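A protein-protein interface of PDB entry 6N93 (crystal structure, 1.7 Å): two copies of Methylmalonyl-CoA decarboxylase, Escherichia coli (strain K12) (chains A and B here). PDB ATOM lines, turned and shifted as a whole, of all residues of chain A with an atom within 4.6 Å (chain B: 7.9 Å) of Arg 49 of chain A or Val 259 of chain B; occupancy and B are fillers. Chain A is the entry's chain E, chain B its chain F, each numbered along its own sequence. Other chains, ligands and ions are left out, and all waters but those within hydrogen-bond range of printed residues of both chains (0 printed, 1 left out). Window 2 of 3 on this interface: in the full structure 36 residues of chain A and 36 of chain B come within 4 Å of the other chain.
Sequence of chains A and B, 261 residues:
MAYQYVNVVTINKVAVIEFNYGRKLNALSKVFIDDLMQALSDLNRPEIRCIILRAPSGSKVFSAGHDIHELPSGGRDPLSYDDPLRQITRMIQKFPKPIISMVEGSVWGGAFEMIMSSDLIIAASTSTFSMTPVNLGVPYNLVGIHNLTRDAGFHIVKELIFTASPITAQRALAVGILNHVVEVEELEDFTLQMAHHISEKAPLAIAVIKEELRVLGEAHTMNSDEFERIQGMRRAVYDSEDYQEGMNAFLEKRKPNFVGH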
ATOM      1  N   LYS A  13     -34.816   4.300   3.465  1.00  0.00           N
ATOM      2  CA  LYS A  13     -33.619   4.931   2.851  1.00  0.00           C
ATOM      3  C   LYS A  13     -33.926   5.456   1.442  1.00  0.00           C
ATOM      4  O   LYS A  13     -32.997   6.030   0.824  1.00  0.00           O
ATOM      5  CB  LYS A  13     -32.514   3.883   2.886  1.00  0.00           C
ATOM      6  CG  LYS A  13     -32.028   3.548   4.283  1.00  0.00           C
ATOM      7  CD  LYS A  13     -31.323   2.248   4.370  1.00  0.00           C
ATOM      8  CE  LYS A  13     -30.721   1.998   5.729  1.00  0.00           C
ATOM      9  NZ  LYS A  13     -30.259   0.586   5.812  1.00  0.00           N
ATOM     10  N   PRO A  46     -26.781  11.136   5.109  1.00  0.00           N
ATOM     11  CA  PRO A  46     -26.299   9.757   5.191  1.00  0.00           C
ATOM     12  C   PRO A  46     -27.373   8.663   5.184  1.00  0.00           C
ATOM     13  O   PRO A  46     -27.076   7.600   4.694  1.00  0.00           O
ATOM     14  CB  PRO A  46     -25.539   9.654   6.521  1.00  0.00           C
ATOM     15  CG  PRO A  46     -25.304  11.075   6.959  1.00  0.00           C
ATOM     16  CD  PRO A  46     -26.202  11.993   6.154  1.00  0.00           C
ATOM     17  N   GLU A  47     -28.549   8.975   5.733  1.00  0.00           N
ATOM     18  CA  GLU A  47     -29.643   8.000   5.931  1.00  0.00           C
ATOM     19  C   GLU A  47     -30.494   7.875   4.649  1.00  0.00           C
ATOM     20  O   GLU A  47     -31.375   6.992   4.621  1.00  0.00           O
ATOM     21  CB  GLU A  47     -30.525   8.379   7.122  1.00  0.00           C
ATOM     22  CG  GLU A  47     -31.270   9.679   6.982  1.00  0.00           C
ATOM     23  CD  GLU A  47     -30.615  10.967   7.476  1.00  0.00           C
ATOM     24  OE1 GLU A  47     -29.356  11.056   7.578  1.00  0.00           O
ATOM     25  OE2 GLU A  47     -31.380  11.918   7.693  1.00  0.00           O
ATOM     26  N   ILE A  48     -30.274   8.737   3.648  1.00  0.00           N
ATOM     27  CA  ILE A  48     -30.918   8.559   2.312  1.00  0.00           C
ATOM     28  C   ILE A  48     -29.923   7.853   1.399  1.00  0.00           C
ATOM     29  O   ILE A  48     -28.770   8.287   1.343  1.00  0.00           O
ATOM     30  CB  ILE A  48     -31.323   9.891   1.702  1.00  0.00           C
ATOM     31  CG1 ILE A  48     -32.272  10.639   2.653  1.00  0.00           C
ATOM     32  CG2 ILE A  48     -31.897   9.698   0.295  1.00  0.00           C
ATOM     33  CD1 ILE A  48     -33.564   9.952   2.864  1.00  0.00           C
ATOM     34  N   ARG A  49     -30.372   6.809   0.723  1.00  0.00           N
ATOM     35  CA  ARG A  49     -29.425   5.972  -0.068  1.00  0.00           C
ATOM     36  C   ARG A  49     -29.781   5.924  -1.553  1.00  0.00           C
ATOM     37  O   ARG A  49     -28.938   5.482  -2.307  1.00  0.00           O
ATOM     38  CB  ARG A  49     -29.381   4.572   0.507  1.00  0.00           C
ATOM     39  CG  ARG A  49     -28.954   4.527   1.971  1.00  0.00           C
ATOM     40  CD  ARG A  49     -27.601   5.077   2.278  1.00  0.00           C
ATOM     41  NE  ARG A  49     -27.286   4.736   3.654  1.00  0.00           N
ATOM     42  CZ  ARG A  49     -26.966   3.520   4.097  1.00  0.00           C
ATOM     43  NH1 ARG A  49     -26.839   2.486   3.283  1.00  0.00           N
ATOM     44  NH2 ARG A  49     -26.795   3.342   5.389  1.00  0.00           N
ATOM     45  N   CYS A  50     -30.972   6.331  -1.951  1.00  0.00           N
ATOM     46  CA  CYS A  50     -31.439   6.163  -3.347  1.00  0.00           C
ATOM     47  C   CYS A  50     -32.561   7.150  -3.587  1.00  0.00           C
ATOM     48  O   CYS A  50     -33.423   7.286  -2.692  1.00  0.00           O
ATOM     49  CB  CYS A  50     -31.870   4.731  -3.626  1.00  0.00           C
ATOM     50  SG  CYS A  50     -32.058   4.343  -5.388  1.00  0.00           S
ATOM     51  N   LYS A  97     -25.552   9.594  -4.531  1.00  0.00           N
ATOM     52  CA  LYS A  97     -26.501   8.481  -4.418  1.00  0.00           C
ATOM     53  C   LYS A  97     -27.054   8.212  -5.795  1.00  0.00           C
ATOM     54  O   LYS A  97     -27.139   9.102  -6.619  1.00  0.00           O
ATOM     55  CB  LYS A  97     -27.609   8.852  -3.446  1.00  0.00           C
ATOM     56  CG  LYS A  97     -27.080   9.309  -2.079  1.00  0.00           C
ATOM     57  CD  LYS A  97     -28.076  10.005  -1.267  1.00  0.00           C
ATOM     58  CE  LYS A  97     -27.451  10.862  -0.178  1.00  0.00           C
ATOM     59  NZ  LYS A  97     -26.727  10.029   0.814  1.00  0.00           N
ATOM     60  N   PRO A  98     -27.460   6.977  -6.074  1.00  0.00           N
ATOM     61  CA  PRO A  98     -28.153   6.678  -7.323  1.00  0.00           C
ATOM     62  C   PRO A  98     -29.466   7.445  -7.448  1.00  0.00           C
ATOM     63  O   PRO A  98     -30.216   7.568  -6.452  1.00  0.00           O
ATOM     64  CB  PRO A  98     -28.408   5.181  -7.252  1.00  0.00           C
ATOM     65  CG  PRO A  98     -27.438   4.717  -6.266  1.00  0.00           C
ATOM     66  CD  PRO A  98     -27.375   5.801  -5.210  1.00  0.00           C
ATOM     67  N   SER A 199     -30.407   0.270  -1.584  1.00  0.00           N
ATOM     68  CA  SER A 199     -30.182   1.003  -0.311  1.00  0.00           C
ATOM     69  C   SER A 199     -29.606   0.076   0.766  1.00  0.00           C
ATOM     70  O   SER A 199     -29.180   0.615   1.804  1.00  0.00           O
ATOM     71  CB  SER A 199     -31.443   1.732   0.182  1.00  0.00           C
ATOM     72  OG  SER A 199     -31.936   2.639  -0.777  1.00  0.00           O
ATOM     73  N   LYS A 201     -26.960  -1.810   0.112  1.00  0.00           N
ATOM     74  CA  LYS A 201     -25.552  -1.961  -0.339  1.00  0.00           C
ATOM     75  C   LYS A 201     -24.709  -0.832   0.241  1.00  0.00           C
ATOM     76  O   LYS A 201     -25.257   0.110   0.799  1.00  0.00           O
ATOM     77  CB  LYS A 201     -25.548  -1.941  -1.874  1.00  0.00           C
ATOM     78  CG  LYS A 201     -26.460  -2.961  -2.529  1.00  0.00           C
ATOM     79  CD  LYS A 201     -26.213  -4.396  -2.071  1.00  0.00           C
ATOM     80  CE  LYS A 201     -26.976  -5.422  -2.882  1.00  0.00           C
ATOM     81  NZ  LYS A 201     -26.686  -6.798  -2.409  1.00  0.00           N
ATOM     82  N   PRO A 203     -22.990   2.418   0.707  1.00  0.00           N
ATOM     83  CA  PRO A 203     -23.183   3.714   0.049  1.00  0.00           C
ATOM     84  C   PRO A 203     -21.884   4.406  -0.404  1.00  0.00           C
ATOM     85  O   PRO A 203     -21.887   5.113  -1.386  1.00  0.00           O
ATOM     86  CB  PRO A 203     -23.871   4.562   1.110  1.00  0.00           C
ATOM     87  CG  PRO A 203     -23.425   3.940   2.409  1.00  0.00           C
ATOM     88  CD  PRO A 203     -23.385   2.453   2.125  1.00  0.00           C
ATOM     89  N   GLU B 241     -15.224   2.562   8.119  1.00  0.00           N
ATOM     90  CA  GLU B 241     -15.720   1.435   8.963  1.00  0.00           C
ATOM     91  C   GLU B 241     -16.616   0.524   8.120  1.00  0.00           C
ATOM     92  O   GLU B 241     -16.585  -0.689   8.351  1.00  0.00           O
ATOM     93  CB  GLU B 241     -16.374   1.943  10.241  1.00  0.00           C
ATOM     94  CG  GLU B 241     -15.310   2.487  11.203  1.00  0.00           C
ATOM     95  CD  GLU B 241     -15.775   3.075  12.525  1.00  0.00           C
ATOM     96  OE1 GLU B 241     -16.441   4.126  12.488  1.00  0.00           O
ATOM     97  OE2 GLU B 241     -15.415   2.522  13.592  1.00  0.00           O
ATOM     98  N   ASP B 242     -17.320   1.076   7.132  1.00  0.00           N
ATOM     99  CA  ASP B 242     -18.179   0.297   6.195  1.00  0.00           C
ATOM    100  C   ASP B 242     -17.368  -0.753   5.453  1.00  0.00           C
ATOM    101  O   ASP B 242     -17.835  -1.908   5.329  1.00  0.00           O
ATOM    102  CB  ASP B 242     -18.949   1.198   5.230  1.00  0.00           C
ATOM    103  CG  ASP B 242     -20.281   1.755   5.758  1.00  0.00           C
ATOM    104  OD1 ASP B 242     -20.700   1.444   6.942  1.00  0.00           O
ATOM    105  OD2 ASP B 242     -20.886   2.508   5.009  1.00  0.00           O
ATOM    106  N   GLU B 245     -16.569  -3.573   7.880  1.00  0.00           N
ATOM    107  CA  GLU B 245     -17.842  -4.266   8.160  1.00  0.00           C
ATOM    108  C   GLU B 245     -18.218  -5.149   6.963  1.00  0.00           C
ATOM    109  O   GLU B 245     -18.665  -6.270   7.205  1.00  0.00           O
ATOM    110  CB  GLU B 245     -18.934  -3.259   8.448  1.00  0.00           C
ATOM    111  CG  GLU B 245     -20.337  -3.813   8.369  1.00  0.00           C
ATOM    112  CD  GLU B 245     -20.740  -4.791   9.475  1.00  0.00           C
ATOM    113  OE1 GLU B 245     -19.918  -5.049  10.402  1.00  0.00           O
ATOM    114  OE2 GLU B 245     -21.866  -5.307   9.376  1.00  0.00           O
ATOM    115  N   PRO B 256     -24.164  -7.462   6.093  1.00  0.00           N
ATOM    116  CA  PRO B 256     -23.463  -6.304   6.650  1.00  0.00           C
ATOM    117  C   PRO B 256     -24.477  -5.233   7.055  1.00  0.00           C
ATOM    118  O   PRO B 256     -25.567  -5.155   6.479  1.00  0.00           O
ATOM    119  CB  PRO B 256     -22.560  -5.842   5.495  1.00  0.00           C
ATOM    120  CG  PRO B 256     -23.311  -6.334   4.256  1.00  0.00           C
ATOM    121  CD  PRO B 256     -23.898  -7.669   4.654  1.00  0.00           C
ATOM    122  N   ASN B 257     -24.092  -4.421   8.017  1.00  0.00           N
ATOM    123  CA  ASN B 257     -24.846  -3.195   8.357  1.00  0.00           C
ATOM    124  C   ASN B 257     -23.972  -1.984   8.021  1.00  0.00           C
ATOM    125  O   ASN B 257     -23.100  -1.593   8.828  1.00  0.00           O
ATOM    126  CB  ASN B 257     -25.354  -3.146   9.802  1.00  0.00           C
ATOM    127  CG  ASN B 257     -26.483  -2.131   9.920  1.00  0.00           C
ATOM    128  OD1 ASN B 257     -27.548  -2.298   9.305  1.00  0.00           O
ATOM    129  ND2 ASN B 257     -26.272  -1.074  10.690  1.00  0.00           N
ATOM    130  N   PHE B 258     -24.261  -1.374   6.875  1.00  0.00           N
ATOM    131  CA  PHE B 258     -23.523  -0.200   6.364  1.00  0.00           C
ATOM    132  C   PHE B 258     -24.215   1.054   6.904  1.00  0.00           C
ATOM    133  O   PHE B 258     -25.459   1.138   6.835  1.00  0.00           O
ATOM    134  CB  PHE B 258     -23.455  -0.252   4.832  1.00  0.00           C
ATOM    135  CG  PHE B 258     -22.725  -1.427   4.218  1.00  0.00           C
ATOM    136  CD1 PHE B 258     -21.399  -1.700   4.503  1.00  0.00           C
ATOM    137  CD2 PHE B 258     -23.374  -2.263   3.325  1.00  0.00           C
ATOM    138  CE1 PHE B 258     -20.764  -2.783   3.910  1.00  0.00           C
ATOM    139  CE2 PHE B 258     -22.730  -3.324   2.722  1.00  0.00           C
ATOM    140  CZ  PHE B 258     -21.421  -3.591   3.017  1.00  0.00           C
ATOM    141  N   VAL B 259     -23.431   2.046   7.301  1.00  0.00           N
ATOM    142  CA  VAL B 259     -23.911   3.297   7.938  1.00  0.00           C
ATOM    143  C   VAL B 259     -23.383   4.534   7.225  1.00  0.00           C
ATOM    144  O   VAL B 259     -23.770   5.625   7.630  1.00  0.00           O
ATOM    145  CB  VAL B 259     -23.505   3.338   9.420  1.00  0.00           C
ATOM    146  CG1 VAL B 259     -24.124   2.162  10.169  1.00  0.00           C
ATOM    147  CG2 VAL B 259     -21.997   3.390   9.620  1.00  0.00           C
ATOM    148  N   GLY B 260     -22.489   4.410   6.244  1.00  0.00           N
ATOM    149  CA  GLY B 260     -22.043   5.621   5.520  1.00  0.00           C
ATOM    150  C   GLY B 260     -20.839   6.299   6.126  1.00  0.00           C
ATOM    151  O   GLY B 260     -20.582   7.460   5.735  1.00  0.00           O
ATOM    152  N   HIS B 261     -20.015   5.616   6.935  1.00  0.00           N
ATOM    153  CA  HIS B 261     -18.649   6.108   7.296  1.00  0.00           C
ATOM    154  C   HIS B 261     -17.740   4.907   7.544  1.00  0.00           C
ATOM    155  O   HIS B 261     -18.256   3.779   7.380  1.00  0.00           O
ATOM    156  CB  HIS B 261     -18.662   7.105   8.469  1.00  0.00           C
ATOM    157  CG  HIS B 261     -19.021   6.489   9.785  1.00  0.00           C
ATOM    158  ND1 HIS B 261     -20.327   6.472  10.249  1.00  0.00           N
ATOM    159  CD2 HIS B 261     -18.275   5.906  10.756  1.00  0.00           C
ATOM    160  CE1 HIS B 261     -20.368   5.920  11.441  1.00  0.00           C
ATOM    161  NE2 HIS B 261     -19.136   5.528  11.766  1.00  0.00           N
ATOM    162  OXT HIS B 261     -16.545   5.054   7.878  1.00  0.00           O
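NH2 of Arg 49 of chain A is in hydrogen-bond range of O of Phe 258 of chain B (3.0 Å).
The backbone NH of Arg 49 of chain A is in hydrogen-bond range of the backbone carbonyl oxygen of Lys 13 of chain A (2.7 Å). The backbone carbonyl oxygen of Pro 46 of chain A lies within hydrogen-bond range of the guanidinium group of Arg 49 of chain A (3.1 Å). O of Ser 199 of chain A is in hydrogen-bond range of NH1 of Arg 49 of chain A (3.3 Å). The backbone NH (N) of Val 259 of chain B is in hydrogen-bond range of the side-chain carboxylate (OD1) of Asp 242 of chain B, at 2.8 Å. OD2 of Asp 242 of chain B is in hydrogen-bond range of N of Gly 260 of chain B. N of Asp 242 of chain B lies within hydrogen-bond range of O of His 261 of chain B, 2.9 Å away.
NH2 of Arg 49 of chain A touches CA of Val 259 of chain B, 3.8 Å away. Lys 201 of chain A touches Phe 258 of chain B (C to CD2, 3.7 Å). Asp 242 of chain B touches Pro 203 of chain A (OD2 to CD, 3.8 Å). Pro 203 of chain A touches Phe 258 of chain B. Pro 203 of chain A touches Gly 260 of chain B (CG to CA, 3.8 Å).
Glu 47 of chain A touches none of the printed residues of chain B. Arg 49 of chain A touches just these residues of chain B: Phe 258 (3.0 Å) and Val 259 (3.8 Å). Of the printed residues of chain B, Lys 201 of chain A touches Phe 258 (3.7 Å). Of the printed residues of chain B, Pro 203 of chain A touches Asp 242 (3.8 Å), Phe 258 (3.8 Å) and Gly 260 (3.8 Å). Of the printed residues of chain A, Phe 258 of chain B touches Arg 49 (3.0 Å), Lys 201 (3.7 Å) and Pro 203 (3.8 Å). Val 259 of chain B touches one residue of chain A. Printed residues of chain A within 4 Å of Gly 260 of chain B: Pro 203 (3.8 Å). The nearest residue of chain B that does not touch Arg 49 of chain A is Gly 260 of chain B (4.5 Å). The nearest residue of chain A that does not touch Val 259 of chain B is Pro 46 of chain A (4.5 Å).
Of the 9 printed residues of chain B, 4 touch a printed residue of chain A. Hydrophobic or aromatic side chains of chain B that line the printed part of chain A: Phe 258. Along chain B the printed residues that touch a printed residue of chain A span positions 242 to 260. Printed residues of chain A that touch a printed residue of chain B: Arg 49, Lys 201 and Pro 203. Among the printed residues, no Asp or Glu carboxylate lies within 4 Å of a Lys or Arg side-chain nitrogen of the other chain.
No position is printed for both chains.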
